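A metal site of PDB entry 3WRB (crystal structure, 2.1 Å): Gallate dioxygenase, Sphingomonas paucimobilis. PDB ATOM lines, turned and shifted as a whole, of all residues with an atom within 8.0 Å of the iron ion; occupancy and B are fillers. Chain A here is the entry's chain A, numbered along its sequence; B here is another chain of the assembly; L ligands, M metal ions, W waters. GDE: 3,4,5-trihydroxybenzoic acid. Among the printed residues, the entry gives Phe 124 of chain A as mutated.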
ATOM      1  N   SER A  11      10.356 -19.173  28.935  1.00  0.00           N
ATOM      2  CA  SER A  11      10.374 -18.412  27.690  1.00  0.00           C
ATOM      3  C   SER A  11       9.014 -17.758  27.466  1.00  0.00           C
ATOM      4  O   SER A  11       7.989 -18.285  27.922  1.00  0.00           O
ATOM      5  CB  SER A  11      10.695 -19.349  26.519  1.00  0.00           C
ATOM      6  OG  SER A  11      12.030 -19.828  26.579  1.00  0.00           O
ATOM      7  N   HIS A  12       8.973 -16.623  26.772  1.00  0.00           N
ATOM      8  CA  HIS A  12       7.664 -16.041  26.459  1.00  0.00           C
ATOM      9  C   HIS A  12       7.350 -15.874  24.982  1.00  0.00           C
ATOM     10  O   HIS A  12       6.363 -15.220  24.643  1.00  0.00           O
ATOM     11  CB  HIS A  12       7.342 -14.770  27.274  1.00  0.00           C
ATOM     12  CG  HIS A  12       8.249 -13.610  27.037  1.00  0.00           C
ATOM     13  ND1 HIS A  12       8.623 -12.743  28.051  1.00  0.00           N
ATOM     14  CD2 HIS A  12       8.837 -13.135  25.906  1.00  0.00           C
ATOM     15  CE1 HIS A  12       9.411 -11.806  27.559  1.00  0.00           C
ATOM     16  NE2 HIS A  12       9.561 -12.023  26.265  1.00  0.00           N
ATOM     17  N   THR A  13       8.140 -16.498  24.111  1.00  0.00           N
ATOM     18  CA  THR A  13       7.891 -16.481  22.667  1.00  0.00           C
ATOM     19  C   THR A  13       6.416 -16.749  22.341  1.00  0.00           C
ATOM     20  O   THR A  13       5.786 -17.620  22.959  1.00  0.00           O
ATOM     21  CB  THR A  13       8.791 -17.485  21.874  1.00  0.00           C
ATOM     22  OG1 THR A  13       8.226 -17.679  20.570  1.00  0.00           O
ATOM     23  CG2 THR A  13       8.868 -18.843  22.572  1.00  0.00           C
ATOM     24  N   PRO A  14       5.871 -16.005  21.349  1.00  0.00           N
ATOM     25  CA  PRO A  14       4.454 -16.097  20.997  1.00  0.00           C
ATOM     26  C   PRO A  14       4.023 -17.473  20.468  1.00  0.00           C
ATOM     27  O   PRO A  14       2.828 -17.737  20.401  1.00  0.00           O
ATOM     28  CB  PRO A  14       4.300 -15.041  19.893  1.00  0.00           C
ATOM     29  CG  PRO A  14       5.650 -14.917  19.293  1.00  0.00           C
ATOM     30  CD  PRO A  14       6.602 -15.089  20.447  1.00  0.00           C
ATOM     31  N   TYR A  56       8.427  -9.248  32.640  1.00  0.00           N
ATOM     32  CA  TYR A  56       8.297  -9.477  31.214  1.00  0.00           C
ATOM     33  C   TYR A  56       8.686  -8.231  30.422  1.00  0.00           C
ATOM     34  O   TYR A  56       8.945  -7.164  31.001  1.00  0.00           O
ATOM     35  CB  TYR A  56       6.848  -9.909  30.866  1.00  0.00           C
ATOM     36  CG  TYR A  56       5.855  -8.764  30.690  1.00  0.00           C
ATOM     37  CD1 TYR A  56       5.387  -8.425  29.426  1.00  0.00           C
ATOM     38  CD2 TYR A  56       5.414  -8.023  31.774  1.00  0.00           C
ATOM     39  CE1 TYR A  56       4.507  -7.378  29.233  1.00  0.00           C
ATOM     40  CE2 TYR A  56       4.508  -6.953  31.586  1.00  0.00           C
ATOM     41  CZ  TYR A  56       4.074  -6.646  30.323  1.00  0.00           C
ATOM     42  OH  TYR A  56       3.187  -5.601  30.103  1.00  0.00           O
ATOM     43  N   ASN A  57       8.738  -8.366  29.098  1.00  0.00           N
ATOM     44  CA  ASN A  57       8.815  -7.172  28.254  1.00  0.00           C
ATOM     45  C   ASN A  57       7.740  -7.154  27.202  1.00  0.00           C
ATOM     46  O   ASN A  57       7.293  -8.213  26.714  1.00  0.00           O
ATOM     47  CB  ASN A  57      10.193  -6.952  27.622  1.00  0.00           C
ATOM     48  CG  ASN A  57      10.409  -7.790  26.390  1.00  0.00           C
ATOM     49  OD1 ASN A  57      10.547  -9.005  26.480  1.00  0.00           O
ATOM     50  ND2 ASN A  57      10.423  -7.162  25.218  1.00  0.00           N
ATOM     51  N   ASP A  58       7.312  -5.939  26.893  1.00  0.00           N
ATOM     52  CA  ASP A  58       6.301  -5.648  25.886  1.00  0.00           C
ATOM     53  C   ASP A  58       7.020  -5.494  24.548  1.00  0.00           C
ATOM     54  O   ASP A  58       8.101  -4.907  24.485  1.00  0.00           O
ATOM     55  CB  ASP A  58       5.545  -4.389  26.310  1.00  0.00           C
ATOM     56  CG  ASP A  58       4.556  -3.910  25.278  1.00  0.00           C
ATOM     57  OD1 ASP A  58       3.380  -4.311  25.345  1.00  0.00           O
ATOM     58  OD2 ASP A  58       4.984  -3.150  24.389  1.00  0.00           O
ATOM     59  N   HIS A  59       6.425  -6.023  23.492  1.00  0.00           N
ATOM     60  CA  HIS A  59       7.118  -6.113  22.207  1.00  0.00           C
ATOM     61  C   HIS A  59       6.593  -5.042  21.274  1.00  0.00           C
ATOM     62  O   HIS A  59       5.972  -5.306  20.237  1.00  0.00           O
ATOM     63  CB  HIS A  59       7.057  -7.550  21.651  1.00  0.00           C
ATOM     64  CG  HIS A  59       7.707  -8.549  22.563  1.00  0.00           C
ATOM     65  ND1 HIS A  59       7.087  -9.075  23.670  1.00  0.00           N
ATOM     66  CD2 HIS A  59       8.963  -9.072  22.561  1.00  0.00           C
ATOM     67  CE1 HIS A  59       7.910  -9.903  24.287  1.00  0.00           C
ATOM     68  NE2 HIS A  59       9.061  -9.906  23.638  1.00  0.00           N
ATOM     69  N   ASP A 123       0.670  -7.793  26.328  1.00  0.00           N
ATOM     70  CA  ASP A 123       0.924  -8.495  25.065  1.00  0.00           C
ATOM     71  C   ASP A 123       1.322  -9.968  25.311  1.00  0.00           C
ATOM     72  O   ASP A 123       1.163 -10.474  26.432  1.00  0.00           O
ATOM     73  CB  ASP A 123       1.951  -7.742  24.188  1.00  0.00           C
ATOM     74  CG  ASP A 123       3.413  -8.076  24.530  1.00  0.00           C
ATOM     75  OD1 ASP A 123       3.709  -8.487  25.696  1.00  0.00           O
ATOM     76  OD2 ASP A 123       4.265  -7.900  23.633  1.00  0.00           O
ATOM     77  N   PHE A 124       1.867 -10.627  24.285  1.00  0.00           N
ATOM     78  CA  PHE A 124       2.291 -12.024  24.398  1.00  0.00           C
ATOM     79  C   PHE A 124       3.392 -12.297  25.430  1.00  0.00           C
ATOM     80  O   PHE A 124       3.524 -13.431  25.898  1.00  0.00           O
ATOM     81  CB  PHE A 124       2.640 -12.632  23.025  1.00  0.00           C
ATOM     82  CG  PHE A 124       3.935 -12.112  22.433  1.00  0.00           C
ATOM     83  CD1 PHE A 124       5.180 -12.585  22.881  1.00  0.00           C
ATOM     84  CD2 PHE A 124       3.907 -11.198  21.373  1.00  0.00           C
ATOM     85  CE1 PHE A 124       6.373 -12.129  22.309  1.00  0.00           C
ATOM     86  CE2 PHE A 124       5.082 -10.742  20.792  1.00  0.00           C
ATOM     87  CZ  PHE A 124       6.318 -11.213  21.256  1.00  0.00           C
ATOM     88  N   GLY A 125       4.176 -11.281  25.766  1.00  0.00           N
ATOM     89  CA  GLY A 125       5.220 -11.410  26.792  1.00  0.00           C
ATOM     90  C   GLY A 125       4.666 -11.927  28.109  1.00  0.00           C
ATOM     91  O   GLY A 125       5.358 -12.632  28.878  1.00  0.00           O
ATOM     92  N   CYS A 149       9.645  -4.510  31.450  1.00  0.00           N
ATOM     93  CA  CYS A 149      11.036  -4.076  31.408  1.00  0.00           C
ATOM     94  C   CYS A 149      11.412  -3.609  30.022  1.00  0.00           C
ATOM     95  O   CYS A 149      11.174  -4.310  29.026  1.00  0.00           O
ATOM     96  CB  CYS A 149      11.948  -5.207  31.872  1.00  0.00           C
ATOM     97  SG  CYS A 149      11.727  -5.643  33.618  1.00  0.00           S
ATOM     98  N   VAL A 151      13.719  -3.533  27.621  1.00  0.00           N
ATOM     99  CA  VAL A 151      14.975  -4.224  27.273  1.00  0.00           C
ATOM    100  C   VAL A 151      15.333  -4.079  25.782  1.00  0.00           C
ATOM    101  O   VAL A 151      16.372  -4.587  25.346  1.00  0.00           O
ATOM    102  CB  VAL A 151      14.943  -5.732  27.653  1.00  0.00           C
ATOM    103  CG1 VAL A 151      14.816  -5.918  29.141  1.00  0.00           C
ATOM    104  CG2 VAL A 151      13.813  -6.484  26.905  1.00  0.00           C
ATOM    105  N   LEU A 152      14.475  -3.385  25.025  1.00  0.00           N
ATOM    106  CA  LEU A 152      14.587  -3.316  23.568  1.00  0.00           C
ATOM    107  C   LEU A 152      15.254  -2.062  22.977  1.00  0.00           C
ATOM    108  O   LEU A 152      15.701  -2.106  21.825  1.00  0.00           O
ATOM    109  CB  LEU A 152      13.194  -3.491  22.929  1.00  0.00           C
ATOM    110  CG  LEU A 152      12.401  -4.763  23.211  1.00  0.00           C
ATOM    111  CD1 LEU A 152      11.034  -4.680  22.540  1.00  0.00           C
ATOM    112  CD2 LEU A 152      13.196  -5.999  22.736  1.00  0.00           C
ATOM    113  N   THR A 187      10.588 -13.996  32.694  1.00  0.00           N
ATOM    114  CA  THR A 187      10.234 -14.581  31.411  1.00  0.00           C
ATOM    115  C   THR A 187      11.077 -14.072  30.233  1.00  0.00           C
ATOM    116  O   THR A 187      11.883 -13.157  30.388  1.00  0.00           O
ATOM    117  CB  THR A 187       8.727 -14.421  31.113  1.00  0.00           C
ATOM    118  OG1 THR A 187       8.421 -13.048  30.828  1.00  0.00           O
ATOM    119  CG2 THR A 187       7.882 -14.937  32.314  1.00  0.00           C
ATOM    120  N   GLY A 188      10.891 -14.694  29.060  1.00  0.00           N
ATOM    121  CA  GLY A 188      11.694 -14.396  27.877  1.00  0.00           C
ATOM    122  C   GLY A 188      12.860 -15.369  27.759  1.00  0.00           C
ATOM    123  O   GLY A 188      13.021 -16.265  28.580  1.00  0.00           O
ATOM    124  N   GLY A 189      13.686 -15.175  26.741  1.00  0.00           N
ATOM    125  CA  GLY A 189      14.824 -16.067  26.528  1.00  0.00           C
ATOM    126  C   GLY A 189      14.383 -17.417  25.955  1.00  0.00           C
ATOM    127  O   GLY A 189      13.212 -17.601  25.614  1.00  0.00           O
ATOM    128  N   HIS A 192      18.270 -16.580  21.128  1.00  0.00           N
ATOM    129  CA  HIS A 192      17.595 -16.374  19.848  1.00  0.00           C
ATOM    130  C   HIS A 192      17.935 -15.013  19.267  1.00  0.00           C
ATOM    131  O   HIS A 192      18.404 -14.111  19.985  1.00  0.00           O
ATOM    132  CB  HIS A 192      16.069 -16.544  19.941  1.00  0.00           C
ATOM    133  CG  HIS A 192      15.353 -15.453  20.687  1.00  0.00           C
ATOM    134  ND1 HIS A 192      15.452 -15.311  22.049  1.00  0.00           N
ATOM    135  CD2 HIS A 192      14.519 -14.474  20.251  1.00  0.00           C
ATOM    136  CE1 HIS A 192      14.697 -14.288  22.436  1.00  0.00           C
ATOM    137  NE2 HIS A 192      14.128 -13.762  21.368  1.00  0.00           N
ATOM    138  N   GLU A 236      18.164 -10.491  20.680  1.00  0.00           N
ATOM    139  CA  GLU A 236      16.968 -10.516  21.515  1.00  0.00           C
ATOM    140  C   GLU A 236      17.124 -11.453  22.696  1.00  0.00           C
ATOM    141  O   GLU A 236      16.483 -11.260  23.742  1.00  0.00           O
ATOM    142  CB  GLU A 236      15.740 -10.832  20.664  1.00  0.00           C
ATOM    143  CG  GLU A 236      15.340  -9.666  19.731  1.00  0.00           C
ATOM    144  CD  GLU A 236      16.138  -9.611  18.440  1.00  0.00           C
ATOM    145  OE1 GLU A 236      16.963 -10.512  18.191  1.00  0.00           O
ATOM    146  OE2 GLU A 236      15.915  -8.659  17.646  1.00  0.00           O
ATOM    147  N   GLY A 237      18.003 -12.446  22.559  1.00  0.00           N
ATOM    148  CA  GLY A 237      18.294 -13.380  23.642  1.00  0.00           C
ATOM    149  C   GLY A 237      18.879 -12.702  24.858  1.00  0.00           C
ATOM    150  O   GLY A 237      18.854 -13.236  25.964  1.00  0.00           O
ATOM    151  N   GLU A 239      17.665 -10.492  26.432  1.00  0.00           N
ATOM    152  CA  GLU A 239      16.578 -10.161  27.349  1.00  0.00           C
ATOM    153  C   GLU A 239      16.643 -11.000  28.651  1.00  0.00           C
ATOM    154  O   GLU A 239      15.888 -10.730  29.611  1.00  0.00           O
ATOM    155  CB  GLU A 239      15.199 -10.281  26.664  1.00  0.00           C
ATOM    156  CG  GLU A 239      14.713 -11.720  26.460  1.00  0.00           C
ATOM    157  CD  GLU A 239      13.388 -11.834  25.758  1.00  0.00           C
ATOM    158  OE1 GLU A 239      12.556 -10.914  25.897  1.00  0.00           O
ATOM    159  OE2 GLU A 239      13.145 -12.854  25.068  1.00  0.00           O
ATOM    160  N   VAL A 240      17.564 -11.964  28.706  1.00  0.00           N
ATOM    161  CA  VAL A 240      17.718 -12.818  29.909  1.00  0.00           C
ATOM    162  C   VAL A 240      18.078 -12.081  31.199  1.00  0.00           C
ATOM    163  O   VAL A 240      18.083 -12.680  32.274  1.00  0.00           O
ATOM    164  CB  VAL A 240      18.695 -14.003  29.703  1.00  0.00           C
ATOM    165  CG1 VAL A 240      18.148 -14.965  28.673  1.00  0.00           C
ATOM    166  CG2 VAL A 240      20.096 -13.527  29.314  1.00  0.00           C
ATOM    167  N   MET A 242      16.202 -10.184  32.573  1.00  0.00           N
ATOM    168  CA  MET A 242      14.934 -10.319  33.290  1.00  0.00           C
ATOM    169  C   MET A 242      14.876 -11.559  34.185  1.00  0.00           C
ATOM    170  O   MET A 242      14.272 -11.536  35.251  1.00  0.00           O
ATOM    171  CB  MET A 242      13.755 -10.279  32.304  1.00  0.00           C
ATOM    172  CG  MET A 242      13.464  -8.888  31.724  1.00  0.00           C
ATOM    173  SD  MET A 242      11.991  -8.840  30.688  1.00  0.00           S
ATOM    174  CE  MET A 242      12.508  -9.785  29.247  1.00  0.00           C
ATOM    175  N   PHE B 374       9.749  -5.978  15.829  1.00  0.00           N
ATOM    176  CA  PHE B 374       8.407  -6.134  16.415  1.00  0.00           C
ATOM    177  C   PHE B 374       7.303  -5.375  15.685  1.00  0.00           C
ATOM    178  O   PHE B 374       6.127  -5.732  15.792  1.00  0.00           O
ATOM    179  CB  PHE B 374       8.453  -5.902  17.931  1.00  0.00           C
ATOM    180  CG  PHE B 374       9.451  -6.772  18.605  1.00  0.00           C
ATOM    181  CD1 PHE B 374       9.232  -8.161  18.703  1.00  0.00           C
ATOM    182  CD2 PHE B 374      10.651  -6.265  19.068  1.00  0.00           C
ATOM    183  CE1 PHE B 374      10.173  -8.997  19.294  1.00  0.00           C
ATOM    184  CE2 PHE B 374      11.610  -7.091  19.668  1.00  0.00           C
ATOM    185  CZ  PHE B 374      11.360  -8.457  19.781  1.00  0.00           C
HETATM  186  OAA GDE L   1       9.456 -17.657  16.549  1.00  0.00           O
HETATM  187  OAB GDE L   1       8.461 -16.187  15.278  1.00  0.00           O
HETATM  188  OAC GDE L   1      11.388 -15.183  20.444  1.00  0.00           O
HETATM  189  OAD GDE L   1       8.255 -12.123  18.516  1.00  0.00           O
HETATM  190  OAE GDE L   1      10.055 -12.743  20.457  1.00  0.00           O
HETATM  191  CAF GDE L   1      10.225 -15.778  18.434  1.00  0.00           C
HETATM  192  CAG GDE L   1       8.629 -14.250  17.441  1.00  0.00           C
HETATM  193  CAH GDE L   1       9.052 -16.503  16.342  1.00  0.00           C
HETATM  194  CAI GDE L   1      10.480 -14.864  19.456  1.00  0.00           C
HETATM  195  CAJ GDE L   1       8.892 -13.326  18.468  1.00  0.00           C
HETATM  196  CAK GDE L   1       9.304 -15.481  17.430  1.00  0.00           C
HETATM  197  CAL GDE L   1       9.813 -13.643  19.474  1.00  0.00           C
HETATM  198 FE    FE M   1      10.726 -10.652  24.921  1.00  0.00          FE
HETATM  199  O   HOH W   1      11.132 -12.240  23.631  1.00  0.00           O
HETATM  200  O   HOH W   2      12.078  -9.434  23.264  1.00  0.00           O
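Water W1 lies within hydrogen-bond range of the side-chain carboxylate of Glu 239 (2.5 Å) and an oxygen (OAE) of the ligand (3.4 Å).
The iron ion is bound by water W1 (2.1 Å).
The side-chain carboxylate (OE1) of Glu 239 binds the iron ion (2.1 Å).
The iron ion is bound by NE2 of His 59, at 2.2 Å.
NE2 of His 12 is bound to the iron ion (2.2 Å).
The iron ion is bound by the side-chain amide oxygen (OD1) of Asn 57, at 2.3 Å.
Water W2 binds the iron ion.
An oxygen (OAC) of the ligand lies close to a ring nitrogen (NE2) of His 192, 3.2 Å away.
The nearest printed residue that does not touch the iron ion is Met 242 (4.8 Å).
A ring nitrogen (ND1) of His 12 sits close to the backbone carbonyl oxygen (O) of Gly 125 (3.4 Å).
OD2 of Asp 123 is in hydrogen-bond range of N of His 59, 2.9 Å away.
The backbone NH of Gly 188 sits at hydrogen-bond distance from a ring nitrogen (ND1) of His 12.
SD of Met 242 lies within hydrogen-bond range of N of Asn 57.
The side-chain carboxylate (OE2) of Glu 239 is in hydrogen-bond range of the backbone NH (N) of Gly 189 (2.9 Å).
A ring nitrogen (ND1) of His 12 is in hydrogen-bond range of the side-chain hydroxyl of Thr 187, at 2.8 Å.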
